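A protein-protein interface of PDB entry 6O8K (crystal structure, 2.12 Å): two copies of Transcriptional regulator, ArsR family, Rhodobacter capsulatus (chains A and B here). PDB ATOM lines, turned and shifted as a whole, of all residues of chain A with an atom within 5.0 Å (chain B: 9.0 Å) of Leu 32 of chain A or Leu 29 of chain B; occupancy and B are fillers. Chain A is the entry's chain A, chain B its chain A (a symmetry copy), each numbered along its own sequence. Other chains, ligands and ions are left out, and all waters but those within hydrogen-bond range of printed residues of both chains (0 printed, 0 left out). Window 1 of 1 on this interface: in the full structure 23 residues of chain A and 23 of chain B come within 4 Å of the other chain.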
ATOM      1  N   LEU A  28      18.430  29.596  14.725  1.00  0.00           N
ATOM      2  CA  LEU A  28      18.622  28.145  14.715  1.00  0.00           C
ATOM      3  C   LEU A  28      20.107  27.799  14.755  1.00  0.00           C
ATOM      4  O   LEU A  28      20.546  26.953  15.544  1.00  0.00           O
ATOM      5  CB  LEU A  28      17.966  27.509  13.482  1.00  0.00           C
ATOM      6  CG  LEU A  28      18.318  26.036  13.217  1.00  0.00           C
ATOM      7  CD1 LEU A  28      17.863  25.183  14.396  1.00  0.00           C
ATOM      8  CD2 LEU A  28      17.654  25.546  11.927  1.00  0.00           C
ATOM      9  N   LEU A  29      20.894  28.433  13.893  1.00  0.00           N
ATOM     10  CA  LEU A  29      22.320  28.135  13.867  1.00  0.00           C
ATOM     11  C   LEU A  29      22.938  28.425  15.231  1.00  0.00           C
ATOM     12  O   LEU A  29      23.738  27.635  15.741  1.00  0.00           O
ATOM     13  CB  LEU A  29      23.018  28.945  12.759  1.00  0.00           C
ATOM     14  CG  LEU A  29      22.531  28.660  11.332  1.00  0.00           C
ATOM     15  CD1 LEU A  29      23.418  29.345  10.312  1.00  0.00           C
ATOM     16  CD2 LEU A  29      22.480  27.150  11.083  1.00  0.00           C
ATOM     17  N   LYS A  30      22.574  29.561  15.831  1.00  0.00           N
ATOM     18  CA  LYS A  30      23.007  29.873  17.188  1.00  0.00           C
ATOM     19  C   LYS A  30      22.712  28.706  18.114  1.00  0.00           C
ATOM     20  O   LYS A  30      23.569  28.278  18.894  1.00  0.00           O
ATOM     21  CB  LYS A  30      22.307  31.142  17.695  1.00  0.00           C
ATOM     22  CG  LYS A  30      23.006  32.442  17.363  1.00  0.00           C
ATOM     23  CD  LYS A  30      22.026  33.635  17.446  1.00  0.00           C
ATOM     24  CE  LYS A  30      22.640  34.951  16.923  1.00  0.00           C
ATOM     25  NZ  LYS A  30      21.656  35.764  16.132  1.00  0.00           N
ATOM     26  N   ALA A  31      21.490  28.175  18.044  1.00  0.00           N
ATOM     27  CA  ALA A  31      21.156  27.073  18.936  1.00  0.00           C
ATOM     28  C   ALA A  31      21.971  25.828  18.608  1.00  0.00           C
ATOM     29  O   ALA A  31      22.237  25.010  19.487  1.00  0.00           O
ATOM     30  CB  ALA A  31      19.666  26.774  18.871  1.00  0.00           C
ATOM     31  N   LEU A  32      22.388  25.660  17.366  1.00  0.00           N
ATOM     32  CA  LEU A  32      23.133  24.446  17.049  1.00  0.00           C
ATOM     33  C   LEU A  32      24.626  24.596  17.272  1.00  0.00           C
ATOM     34  O   LEU A  32      25.341  23.586  17.310  1.00  0.00           O
ATOM     35  CB  LEU A  32      22.898  24.028  15.595  1.00  0.00           C
ATOM     36  CG  LEU A  32      21.472  23.744  15.155  1.00  0.00           C
ATOM     37  CD1 LEU A  32      21.404  23.613  13.616  1.00  0.00           C
ATOM     38  CD2 LEU A  32      20.945  22.503  15.876  1.00  0.00           C
ATOM     39  N   ALA A  33      25.119  25.823  17.395  1.00  0.00           N
ATOM     40  CA  ALA A  33      26.564  26.062  17.364  1.00  0.00           C
ATOM     41  C   ALA A  33      27.186  25.868  18.754  1.00  0.00           C
ATOM     42  O   ALA A  33      27.786  26.772  19.342  1.00  0.00           O
ATOM     43  CB  ALA A  33      26.851  27.450  16.800  1.00  0.00           C
ATOM     44  N   HIS A  34      27.026  24.650  19.270  1.00  0.00           N
ATOM     45  CA  HIS A  34      27.539  24.269  20.581  1.00  0.00           C
ATOM     46  C   HIS A  34      27.976  22.821  20.478  1.00  0.00           C
ATOM     47  O   HIS A  34      27.184  21.962  20.078  1.00  0.00           O
ATOM     48  CB  HIS A  34      26.482  24.438  21.689  1.00  0.00           C
ATOM     49  CG  HIS A  34      25.898  25.819  21.765  1.00  0.00           C
ATOM     50  ND1 HIS A  34      26.537  26.865  22.392  1.00  0.00           N
ATOM     51  CD2 HIS A  34      24.731  26.325  21.296  1.00  0.00           C
ATOM     52  CE1 HIS A  34      25.797  27.956  22.305  1.00  0.00           C
ATOM     53  NE2 HIS A  34      24.695  27.657  21.642  1.00  0.00           N
ATOM     54  N   LEU A  38      25.517  19.932  19.516  1.00  0.00           N
ATOM     55  CA  LEU A  38      25.631  19.525  18.124  1.00  0.00           C
ATOM     56  C   LEU A  38      25.925  18.034  18.023  1.00  0.00           C
ATOM     57  O   LEU A  38      25.363  17.343  17.160  1.00  0.00           O
ATOM     58  CB  LEU A  38      26.712  20.338  17.417  1.00  0.00           C
ATOM     59  CG  LEU A  38      26.854  20.138  15.904  1.00  0.00           C
ATOM     60  CD1 LEU A  38      25.523  20.173  15.135  1.00  0.00           C
ATOM     61  CD2 LEU A  38      27.826  21.214  15.368  1.00  0.00           C
ATOM     62  N   MET A  41      22.879  16.159  18.442  1.00  0.00           N
ATOM     63  CA  MET A  41      22.034  16.274  17.263  1.00  0.00           C
ATOM     64  C   MET A  41      22.533  15.352  16.149  1.00  0.00           C
ATOM     65  O   MET A  41      21.738  14.718  15.453  1.00  0.00           O
ATOM     66  CB  MET A  41      21.972  17.733  16.813  1.00  0.00           C
ATOM     67  CG  MET A  41      21.263  18.657  17.809  1.00  0.00           C
ATOM     68  SD  MET A  41      19.491  18.307  17.961  1.00  0.00           S
ATOM     69  CE  MET A  41      18.951  19.144  16.453  1.00  0.00           C
ATOM     70  N   LEU A  77      14.092  21.200  19.291  1.00  0.00           N
ATOM     71  CA  LEU A  77      14.998  20.540  18.355  1.00  0.00           C
ATOM     72  C   LEU A  77      14.951  19.026  18.477  1.00  0.00           C
ATOM     73  O   LEU A  77      15.205  18.315  17.488  1.00  0.00           O
ATOM     74  CB  LEU A  77      16.420  21.052  18.574  1.00  0.00           C
ATOM     75  CG  LEU A  77      16.558  22.558  18.302  1.00  0.00           C
ATOM     76  CD1 LEU A  77      17.940  23.093  18.698  1.00  0.00           C
ATOM     77  CD2 LEU A  77      16.320  22.820  16.825  1.00  0.00           C
ATOM     78  N   ALA A  96      15.627  22.111  11.467  1.00  0.00           N
ATOM     79  CA  ALA A  96      16.868  21.792  12.173  1.00  0.00           C
ATOM     80  C   ALA A  96      17.378  20.423  11.775  1.00  0.00           C
ATOM     81  O   ALA A  96      18.589  20.228  11.593  1.00  0.00           O
ATOM     82  CB  ALA A  96      16.672  21.838  13.688  1.00  0.00           C
ATOM     83  N   VAL A  99      19.160  20.567   8.490  1.00  0.00           N
ATOM     84  CA  VAL A  99      20.444  21.269   8.625  1.00  0.00           C
ATOM     85  C   VAL A  99      21.469  20.375   9.290  1.00  0.00           C
ATOM     86  O   VAL A  99      22.649  20.360   8.921  1.00  0.00           O
ATOM     87  CB  VAL A  99      20.295  22.561   9.445  1.00  0.00           C
ATOM     88  CG1 VAL A  99      21.710  23.131   9.772  1.00  0.00           C
ATOM     89  CG2 VAL A  99      19.436  23.546   8.715  1.00  0.00           C
ATOM     90  N   VAL A 100      21.038  19.657  10.323  1.00  0.00           N
ATOM     91  CA  VAL A 100      21.922  18.786  11.071  1.00  0.00           C
ATOM     92  C   VAL A 100      22.359  17.625  10.201  1.00  0.00           C
ATOM     93  O   VAL A 100      23.516  17.199  10.257  1.00  0.00           O
ATOM     94  CB  VAL A 100      21.221  18.320  12.356  1.00  0.00           C
ATOM     95  CG1 VAL A 100      21.968  17.163  12.996  1.00  0.00           C
ATOM     96  CG2 VAL A 100      21.085  19.494  13.321  1.00  0.00           C
ATOM     97  N   VAL A 103      25.091  19.089   8.076  1.00  0.00           N
ATOM     98  CA  VAL A 103      26.283  19.261   8.906  1.00  0.00           C
ATOM     99  C   VAL A 103      26.929  17.911   9.208  1.00  0.00           C
ATOM    100  O   VAL A 103      28.157  17.754   9.135  1.00  0.00           O
ATOM    101  CB  VAL A 103      25.954  20.021  10.193  1.00  0.00           C
ATOM    102  CG1 VAL A 103      27.175  19.987  11.105  1.00  0.00           C
ATOM    103  CG2 VAL A 103      25.505  21.478   9.879  1.00  0.00           C
ATOM    104  N   ARG B  21      35.656  17.096  15.274  1.00  0.00           N
ATOM    105  CA  ARG B  21      34.760  17.302  14.103  1.00  0.00           C
ATOM    106  C   ARG B  21      33.576  18.162  14.540  1.00  0.00           C
ATOM    107  O   ARG B  21      33.219  19.087  13.813  1.00  0.00           O
ATOM    108  CB  ARG B  21      34.195  15.984  13.577  1.00  0.00           C
ATOM    109  CG  ARG B  21      35.197  15.058  12.905  1.00  0.00           C
ATOM    110  CD  ARG B  21      35.997  15.665  11.772  1.00  0.00           C
ATOM    111  NE  ARG B  21      36.924  14.734  11.146  1.00  0.00           N
ATOM    112  CZ  ARG B  21      36.640  13.473  10.859  1.00  0.00           C
ATOM    113  NH1 ARG B  21      37.548  12.699  10.291  1.00  0.00           N
ATOM    114  NH2 ARG B  21      35.450  12.984  11.149  1.00  0.00           N
ATOM    115  N   ALA B  22      32.979  17.819  15.675  1.00  0.00           N
ATOM    116  CA  ALA B  22      31.880  18.592  16.222  1.00  0.00           C
ATOM    117  C   ALA B  22      32.332  19.990  16.603  1.00  0.00           C
ATOM    118  O   ALA B  22      31.568  20.944  16.446  1.00  0.00           O
ATOM    119  CB  ALA B  22      31.294  17.862  17.434  1.00  0.00           C
ATOM    120  N   ARG B  23      33.578  20.141  17.053  1.00  0.00           N
ATOM    121  CA  ARG B  23      34.088  21.482  17.312  1.00  0.00           C
ATOM    122  C   ARG B  23      34.248  22.276  16.023  1.00  0.00           C
ATOM    123  O   ARG B  23      33.875  23.458  15.968  1.00  0.00           O
ATOM    124  CB  ARG B  23      35.414  21.429  18.057  1.00  0.00           C
ATOM    125  CG  ARG B  23      35.725  22.748  18.727  1.00  0.00           C
ATOM    126  CD  ARG B  23      37.163  23.189  18.549  1.00  0.00           C
ATOM    127  NE  ARG B  23      37.339  24.530  19.106  1.00  0.00           N
ATOM    128  CZ  ARG B  23      38.100  25.481  18.571  1.00  0.00           C
ATOM    129  NH1 ARG B  23      38.786  25.245  17.458  1.00  0.00           N
ATOM    130  NH2 ARG B  23      38.179  26.669  19.158  1.00  0.00           N
ATOM    131  N   ALA B  24      34.808  21.659  14.976  1.00  0.00           N
ATOM    132  CA  ALA B  24      34.918  22.361  13.693  1.00  0.00           C
ATOM    133  C   ALA B  24      33.545  22.765  13.170  1.00  0.00           C
ATOM    134  O   ALA B  24      33.331  23.900  12.709  1.00  0.00           O
ATOM    135  CB  ALA B  24      35.630  21.489  12.661  1.00  0.00           C
ATOM    136  N   ALA B  25      32.602  21.833  13.219  1.00  0.00           N
ATOM    137  CA  ALA B  25      31.266  22.116  12.719  1.00  0.00           C
ATOM    138  C   ALA B  25      30.623  23.232  13.519  1.00  0.00           C
ATOM    139  O   ALA B  25      30.052  24.166  12.945  1.00  0.00           O
ATOM    140  CB  ALA B  25      30.413  20.849  12.754  1.00  0.00           C
ATOM    141  N   SER B  26      30.706  23.167  14.851  1.00  0.00           N
ATOM    142  CA  SER B  26      30.088  24.234  15.623  1.00  0.00           C
ATOM    143  C   SER B  26      30.799  25.563  15.381  1.00  0.00           C
ATOM    144  O   SER B  26      30.158  26.617  15.394  1.00  0.00           O
ATOM    145  CB  SER B  26      30.050  23.868  17.111  1.00  0.00           C
ATOM    146  OG  SER B  26      31.339  23.850  17.660  1.00  0.00           O
ATOM    147  N   ASN B  27      32.094  25.550  15.084  1.00  0.00           N
ATOM    148  CA  ASN B  27      32.733  26.821  14.744  1.00  0.00           C
ATOM    149  C   ASN B  27      32.203  27.367  13.418  1.00  0.00           C
ATOM    150  O   ASN B  27      31.960  28.575  13.292  1.00  0.00           O
ATOM    151  CB  ASN B  27      34.249  26.656  14.732  1.00  0.00           C
ATOM    152  CG  ASN B  27      34.819  26.524  16.144  1.00  0.00           C
ATOM    153  OD1 ASN B  27      34.246  27.047  17.111  1.00  0.00           O
ATOM    154  ND2 ASN B  27      35.931  25.806  16.272  1.00  0.00           N
ATOM    155  N   LEU B  28      31.970  26.493  12.430  1.00  0.00           N
ATOM    156  CA  LEU B  28      31.342  26.962  11.193  1.00  0.00           C
ATOM    157  C   LEU B  28      29.972  27.567  11.483  1.00  0.00           C
ATOM    158  O   LEU B  28      29.643  28.661  11.009  1.00  0.00           O
ATOM    159  CB  LEU B  28      31.209  25.821  10.176  1.00  0.00           C
ATOM    160  CG  LEU B  28      30.334  26.115   8.946  1.00  0.00           C
ATOM    161  CD1 LEU B  28      30.928  27.281   8.164  1.00  0.00           C
ATOM    162  CD2 LEU B  28      30.231  24.878   8.049  1.00  0.00           C
ATOM    163  N   LEU B  29      29.151  26.855  12.246  1.00  0.00           N
ATOM    164  CA  LEU B  29      27.820  27.369  12.545  1.00  0.00           C
ATOM    165  C   LEU B  29      27.928  28.714  13.254  1.00  0.00           C
ATOM    166  O   LEU B  29      27.195  29.656  12.936  1.00  0.00           O
ATOM    167  CB  LEU B  29      27.032  26.355  13.397  1.00  0.00           C
ATOM    168  CG  LEU B  29      26.787  24.993  12.735  1.00  0.00           C
ATOM    169  CD1 LEU B  29      25.833  24.154  13.561  1.00  0.00           C
ATOM    170  CD2 LEU B  29      26.254  25.185  11.314  1.00  0.00           C
ATOM    171  N   LYS B  30      28.842  28.817  14.223  1.00  0.00           N
ATOM    172  CA  LYS B  30      29.113  30.092  14.877  1.00  0.00           C
ATOM    173  C   LYS B  30      29.369  31.169  13.838  1.00  0.00           C
ATOM    174  O   LYS B  30      28.810  32.269  13.909  1.00  0.00           O
ATOM    175  CB  LYS B  30      30.319  29.964  15.818  1.00  0.00           C
ATOM    176  CG  LYS B  30      29.998  29.514  17.225  1.00  0.00           C
ATOM    177  CD  LYS B  30      31.251  28.936  17.923  1.00  0.00           C
ATOM    178  CE  LYS B  30      30.930  28.281  19.283  1.00  0.00           C
ATOM    179  NZ  LYS B  30      31.716  27.021  19.508  1.00  0.00           N
ATOM    180  N   ALA B  31      30.223  30.871  12.858  1.00  0.00           N
ATOM    181  CA  ALA B  31      30.518  31.887  11.858  1.00  0.00           C
ATOM    182  C   ALA B  31      29.292  32.206  11.011  1.00  0.00           C
ATOM    183  O   ALA B  31      29.157  33.319  10.506  1.00  0.00           O
ATOM    184  CB  ALA B  31      31.679  31.443  10.979  1.00  0.00           C
ATOM    185  N   LEU B  32      28.383  31.263  10.845  1.00  0.00           N
ATOM    186  CA  LEU B  32      27.230  31.560  10.000  1.00  0.00           C
ATOM    187  C   LEU B  32      26.084  32.191  10.767  1.00  0.00           C
ATOM    188  O   LEU B  32      25.164  32.742  10.147  1.00  0.00           O
ATOM    189  CB  LEU B  32      26.716  30.291   9.315  1.00  0.00           C
ATOM    190  CG  LEU B  32      27.675  29.523   8.423  1.00  0.00           C
ATOM    191  CD1 LEU B  32      27.074  28.146   8.052  1.00  0.00           C
ATOM    192  CD2 LEU B  32      28.024  30.364   7.194  1.00  0.00           C
ATOM    193  N   ALA B  33      26.098  32.108  12.093  1.00  0.00           N
ATOM    194  CA  ALA B  33      24.919  32.469  12.885  1.00  0.00           C
ATOM    195  C   ALA B  33      24.881  33.977  13.161  1.00  0.00           C
ATOM    196  O   ALA B  33      24.888  34.441  14.306  1.00  0.00           O
ATOM    197  CB  ALA B  33      24.885  31.652  14.173  1.00  0.00           C
ATOM    198  N   HIS B  34      24.841  34.742  12.071  1.00  0.00           N
ATOM    199  CA  HIS B  34      24.804  36.200  12.123  1.00  0.00           C
ATOM    200  C   HIS B  34      23.929  36.660  10.974  1.00  0.00           C
ATOM    201  O   HIS B  34      24.178  36.294   9.821  1.00  0.00           O
ATOM    202  CB  HIS B  34      26.212  36.819  12.014  1.00  0.00           C
ATOM    203  CG  HIS B  34      27.182  36.307  13.039  1.00  0.00           C
ATOM    204  ND1 HIS B  34      27.215  36.777  14.333  1.00  0.00           N
ATOM    205  CD2 HIS B  34      28.157  35.368  12.960  1.00  0.00           C
ATOM    206  CE1 HIS B  34      28.162  36.151  15.010  1.00  0.00           C
ATOM    207  NE2 HIS B  34      28.747  35.288  14.201  1.00  0.00           N
ATOM    208  N   ARG B  37      25.610  38.451   7.751  1.00  0.00           N
ATOM    209  CA  ARG B  37      26.497  37.527   7.051  1.00  0.00           C
ATOM    210  C   ARG B  37      25.709  36.356   6.473  1.00  0.00           C
ATOM    211  O   ARG B  37      25.947  35.930   5.331  1.00  0.00           O
ATOM    212  CB  ARG B  37      27.596  37.047   8.011  1.00  0.00           C
ATOM    213  CG  ARG B  37      28.785  38.007   8.069  1.00  0.00           C
ATOM    214  CD  ARG B  37      29.695  37.737   9.255  1.00  0.00           C
ATOM    215  NE  ARG B  37      29.175  38.370  10.455  1.00  0.00           N
ATOM    216  CZ  ARG B  37      29.719  38.239  11.655  1.00  0.00           C
ATOM    217  NH1 ARG B  37      30.791  37.485  11.810  1.00  0.00           N
ATOM    218  NH2 ARG B  37      29.190  38.860  12.698  1.00  0.00           N
ATOM    219  N   LEU B  38      24.742  35.838   7.235  1.00  0.00           N
ATOM    220  CA  LEU B  38      23.956  34.733   6.710  1.00  0.00           C
ATOM    221  C   LEU B  38      23.191  35.161   5.465  1.00  0.00           C
ATOM    222  O   LEU B  38      23.108  34.401   4.488  1.00  0.00           O
ATOM    223  CB  LEU B  38      23.001  34.203   7.776  1.00  0.00           C
ATOM    224  CG  LEU B  38      22.208  32.937   7.431  1.00  0.00           C
ATOM    225  CD1 LEU B  38      23.054  31.809   6.816  1.00  0.00           C
ATOM    226  CD2 LEU B  38      21.498  32.452   8.716  1.00  0.00           C
ATOM    227  N   GLU B  75      37.209  34.279   6.878  1.00  0.00           N
ATOM    228  CA  GLU B  75      36.904  32.958   7.406  1.00  0.00           C
ATOM    229  C   GLU B  75      36.841  31.902   6.329  1.00  0.00           C
ATOM    230  O   GLU B  75      36.426  30.776   6.613  1.00  0.00           O
ATOM    231  CB  GLU B  75      35.611  32.998   8.212  1.00  0.00           C
ATOM    232  CG  GLU B  75      35.889  33.684   9.538  1.00  0.00           C
ATOM    233  CD  GLU B  75      34.706  33.755  10.452  1.00  0.00           C
ATOM    234  OE1 GLU B  75      33.667  34.287  10.016  1.00  0.00           O
ATOM    235  OE2 GLU B  75      34.827  33.311  11.615  1.00  0.00           O
ATOM    236  N   LEU B  77      34.871  31.653   3.763  1.00  0.00           N
ATOM    237  CA  LEU B  77      33.509  31.283   3.394  1.00  0.00           C
ATOM    238  C   LEU B  77      33.118  31.812   2.023  1.00  0.00           C
ATOM    239  O   LEU B  77      32.278  31.202   1.338  1.00  0.00           O
ATOM    240  CB  LEU B  77      32.536  31.785   4.459  1.00  0.00           C
ATOM    241  CG  LEU B  77      32.785  31.151   5.837  1.00  0.00           C
ATOM    242  CD1 LEU B  77      31.927  31.794   6.933  1.00  0.00           C
ATOM    243  CD2 LEU B  77      32.480  29.665   5.763  1.00  0.00           C
ATOM    244  N   ARG B  95      32.084  22.796   2.555  1.00  0.00           N
ATOM    245  CA  ARG B  95      31.144  22.430   3.634  1.00  0.00           C
ATOM    246  C   ARG B  95      30.185  23.591   3.897  1.00  0.00           C
ATOM    247  O   ARG B  95      28.994  23.357   3.884  1.00  0.00           O
ATOM    248  CB  ARG B  95      31.930  21.974   4.860  1.00  0.00           C
ATOM    249  CG  ARG B  95      32.979  20.926   4.531  1.00  0.00           C
ATOM    250  CD  ARG B  95      33.866  20.555   5.695  1.00  0.00           C
ATOM    251  NE  ARG B  95      34.592  21.715   6.171  1.00  0.00           N
ATOM    252  CZ  ARG B  95      35.691  21.677   6.906  1.00  0.00           C
ATOM    253  NH1 ARG B  95      36.275  22.803   7.281  1.00  0.00           N
ATOM    254  NH2 ARG B  95      36.209  20.514   7.251  1.00  0.00           N
ATOM    255  N   ALA B  96      30.701  24.804   4.062  1.00  0.00           N
ATOM    256  CA  ALA B  96      29.817  25.927   4.374  1.00  0.00           C
ATOM    257  C   ALA B  96      28.785  26.121   3.284  1.00  0.00           C
ATOM    258  O   ALA B  96      27.610  26.396   3.566  1.00  0.00           O
ATOM    259  CB  ALA B  96      30.608  27.221   4.558  1.00  0.00           C
ATOM    260  N   VAL B  99      25.981  23.673   3.649  1.00  0.00           N
ATOM    261  CA  VAL B  99      25.154  24.001   4.819  1.00  0.00           C
ATOM    262  C   VAL B  99      24.257  25.183   4.519  1.00  0.00           C
ATOM    263  O   VAL B  99      23.090  25.228   4.925  1.00  0.00           O
ATOM    264  CB  VAL B  99      26.020  24.325   6.047  1.00  0.00           C
ATOM    265  CG1 VAL B  99      25.116  24.906   7.178  1.00  0.00           C
ATOM    266  CG2 VAL B  99      26.778  23.111   6.486  1.00  0.00           C
ATOM    267  N   VAL B 100      24.814  26.186   3.848  1.00  0.00           N
ATOM    268  CA  VAL B 100      24.079  27.393   3.525  1.00  0.00           C
ATOM    269  C   VAL B 100      22.986  27.076   2.523  1.00  0.00           C
ATOM    270  O   VAL B 100      21.880  27.615   2.610  1.00  0.00           O
ATOM    271  CB  VAL B 100      25.050  28.465   3.008  1.00  0.00           C
ATOM    272  CG1 VAL B 100      24.298  29.612   2.356  1.00  0.00           C
ATOM    273  CG2 VAL B 100      25.926  28.959   4.156  1.00  0.00           C
ATOM    274  N   VAL B 103      20.249  25.601   4.633  1.00  0.00           N
ATOM    275  CA  VAL B 103      19.612  26.680   5.388  1.00  0.00           C
ATOM    276  C   VAL B 103      18.751  27.544   4.471  1.00  0.00           C
ATOM    277  O   VAL B 103      17.616  27.912   4.810  1.00  0.00           O
ATOM    278  CB  VAL B 103      20.652  27.521   6.131  1.00  0.00           C
ATOM    279  CG1 VAL B 103      19.958  28.743   6.723  1.00  0.00           C
ATOM    280  CG2 VAL B 103      21.374  26.678   7.223  1.00  0.00           C
ATOM    281  N   PHE B 107      14.619  27.655   5.033  1.00  0.00           N
ATOM    282  CA  PHE B 107      13.979  28.872   5.585  1.00  0.00           C
ATOM    283  C   PHE B 107      13.249  29.677   4.515  1.00  0.00           C
ATOM    284  O   PHE B 107      12.902  30.804   4.805  1.00  0.00           O
ATOM    285  CB  PHE B 107      14.967  29.684   6.408  1.00  0.00           C
ATOM    286  CG  PHE B 107      15.209  29.059   7.746  1.00  0.00           C
ATOM    287  CD1 PHE B 107      14.435  29.410   8.831  1.00  0.00           C
ATOM    288  CD2 PHE B 107      16.155  28.072   7.899  1.00  0.00           C
ATOM    289  CE1 PHE B 107      14.630  28.809  10.055  1.00  0.00           C
ATOM    290  CE2 PHE B 107      16.357  27.478   9.126  1.00  0.00           C
ATOM    291  CZ  PHE B 107      15.588  27.845  10.196  1.00  0.00           C
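O of Lys 30 of chain A is in hydrogen-bond range of NE2 of His 34 of chain A (3.0 Å). O of Ala 22 of chain B sits at hydrogen-bond distance from OG of Ser 26 of chain B. O of Arg 23 of chain B lies within hydrogen-bond range of OG of Ser 26 of chain B (3.1 Å). The side-chain amide oxygen (OD1) of Asn 27 of chain B is in hydrogen-bond range of the side-chain amino group (NZ) of Lys 30 of chain B (3.5 Å). The backbone carbonyl oxygen of Lys 30 of chain B lies within hydrogen-bond range of a ring nitrogen (NE2) of His 34 of chain B (3.0 Å).
Ala 33 of chain B touches Lys 30 of chain A. CD1 of Leu 29 of chain B touches CB of Leu 32 of chain A, 3.6 Å away. Ala 33 of chain A touches Leu 29 of chain B. CE of Lys 30 of chain B touches O of Ala 33 of chain A, 3.5 Å away. Ser 26 of chain B touches His 34 of chain A (CB to N, 3.8 Å). CD2 of Leu 38 of chain A touches CB of Ala 25 of chain B (3.7 Å). N of Ser 26 of chain B touches CD2 of Leu 38 of chain A (3.5 Å). Leu 29 of chain B touches Leu 38 of chain A. Val 99 of chain A touches Val 103 of chain B. CG2 of Val 103 of chain A touches CG2 of Val 99 of chain B, at 3.97 Å.
Of chain B, only Leu 29 comes within 4 Å of Leu 32 of chain A. Of the printed residues of chain A, Leu 29 of chain B touches Leu 32 (3.6 Å), Ala 33 (3.6 Å) and Leu 38 (3.99 Å). No residue of chain B comes within 4 Å of Ala 31 of chain A. Of the printed residues of chain B, Val 99 of chain A touches Val 103 (3.97 Å). Of the printed residues of chain A, Lys 30 of chain B touches Ala 33.
Hydrophobic or aromatic side chains of chain A that line the printed part of chain B: Leu 28, Leu 29, Leu 32, Ala 33, Leu 38, Val 99 and Val 103. Along chain A the printed residues that touch a printed residue of chain B span positions 28 to 103. Printed residues of chain B that touch a printed residue of chain A: Ala 22, Ala 25, Ser 26, Leu 29, Lys 30, Leu 32, Ala 33, Leu 38, Val 99, Val 103 and Phe 107. Hydrophobic or aromatic side chains of chain B that line the printed part of chain A: Ala 25, Leu 29, Leu 32, Ala 33, Leu 38, Val 99, Val 103 and Phe 107. Among the printed residues, 17 pairs touch across the chains. Among the printed residues, no Asp or Glu carboxylate lies within 4 Å of a Lys or Arg side-chain nitrogen of the other chain.
Leu 29 of chain A touches Leu 32 of chain B, and with the chains exchanged Leu 32 of chain A touches Leu 29 of chain B. Leu 29 of chain A touches Ala 33 of chain B, and with the chains exchanged Ala 33 of chain A touches Leu 29 of chain B. Leu 29 of chain A touches Leu 38 of chain B, and with the chains exchanged Leu 38 of chain A touches Leu 29 of chain B. Val 99 of chain A touches Val 103 of chain B, and with the chains exchanged Val 103 of chain A touches Val 99 of chain B. Of the 17 pairs that touch across the chains among the printed residues, 10 have their exchanged pair printed and touching as well.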
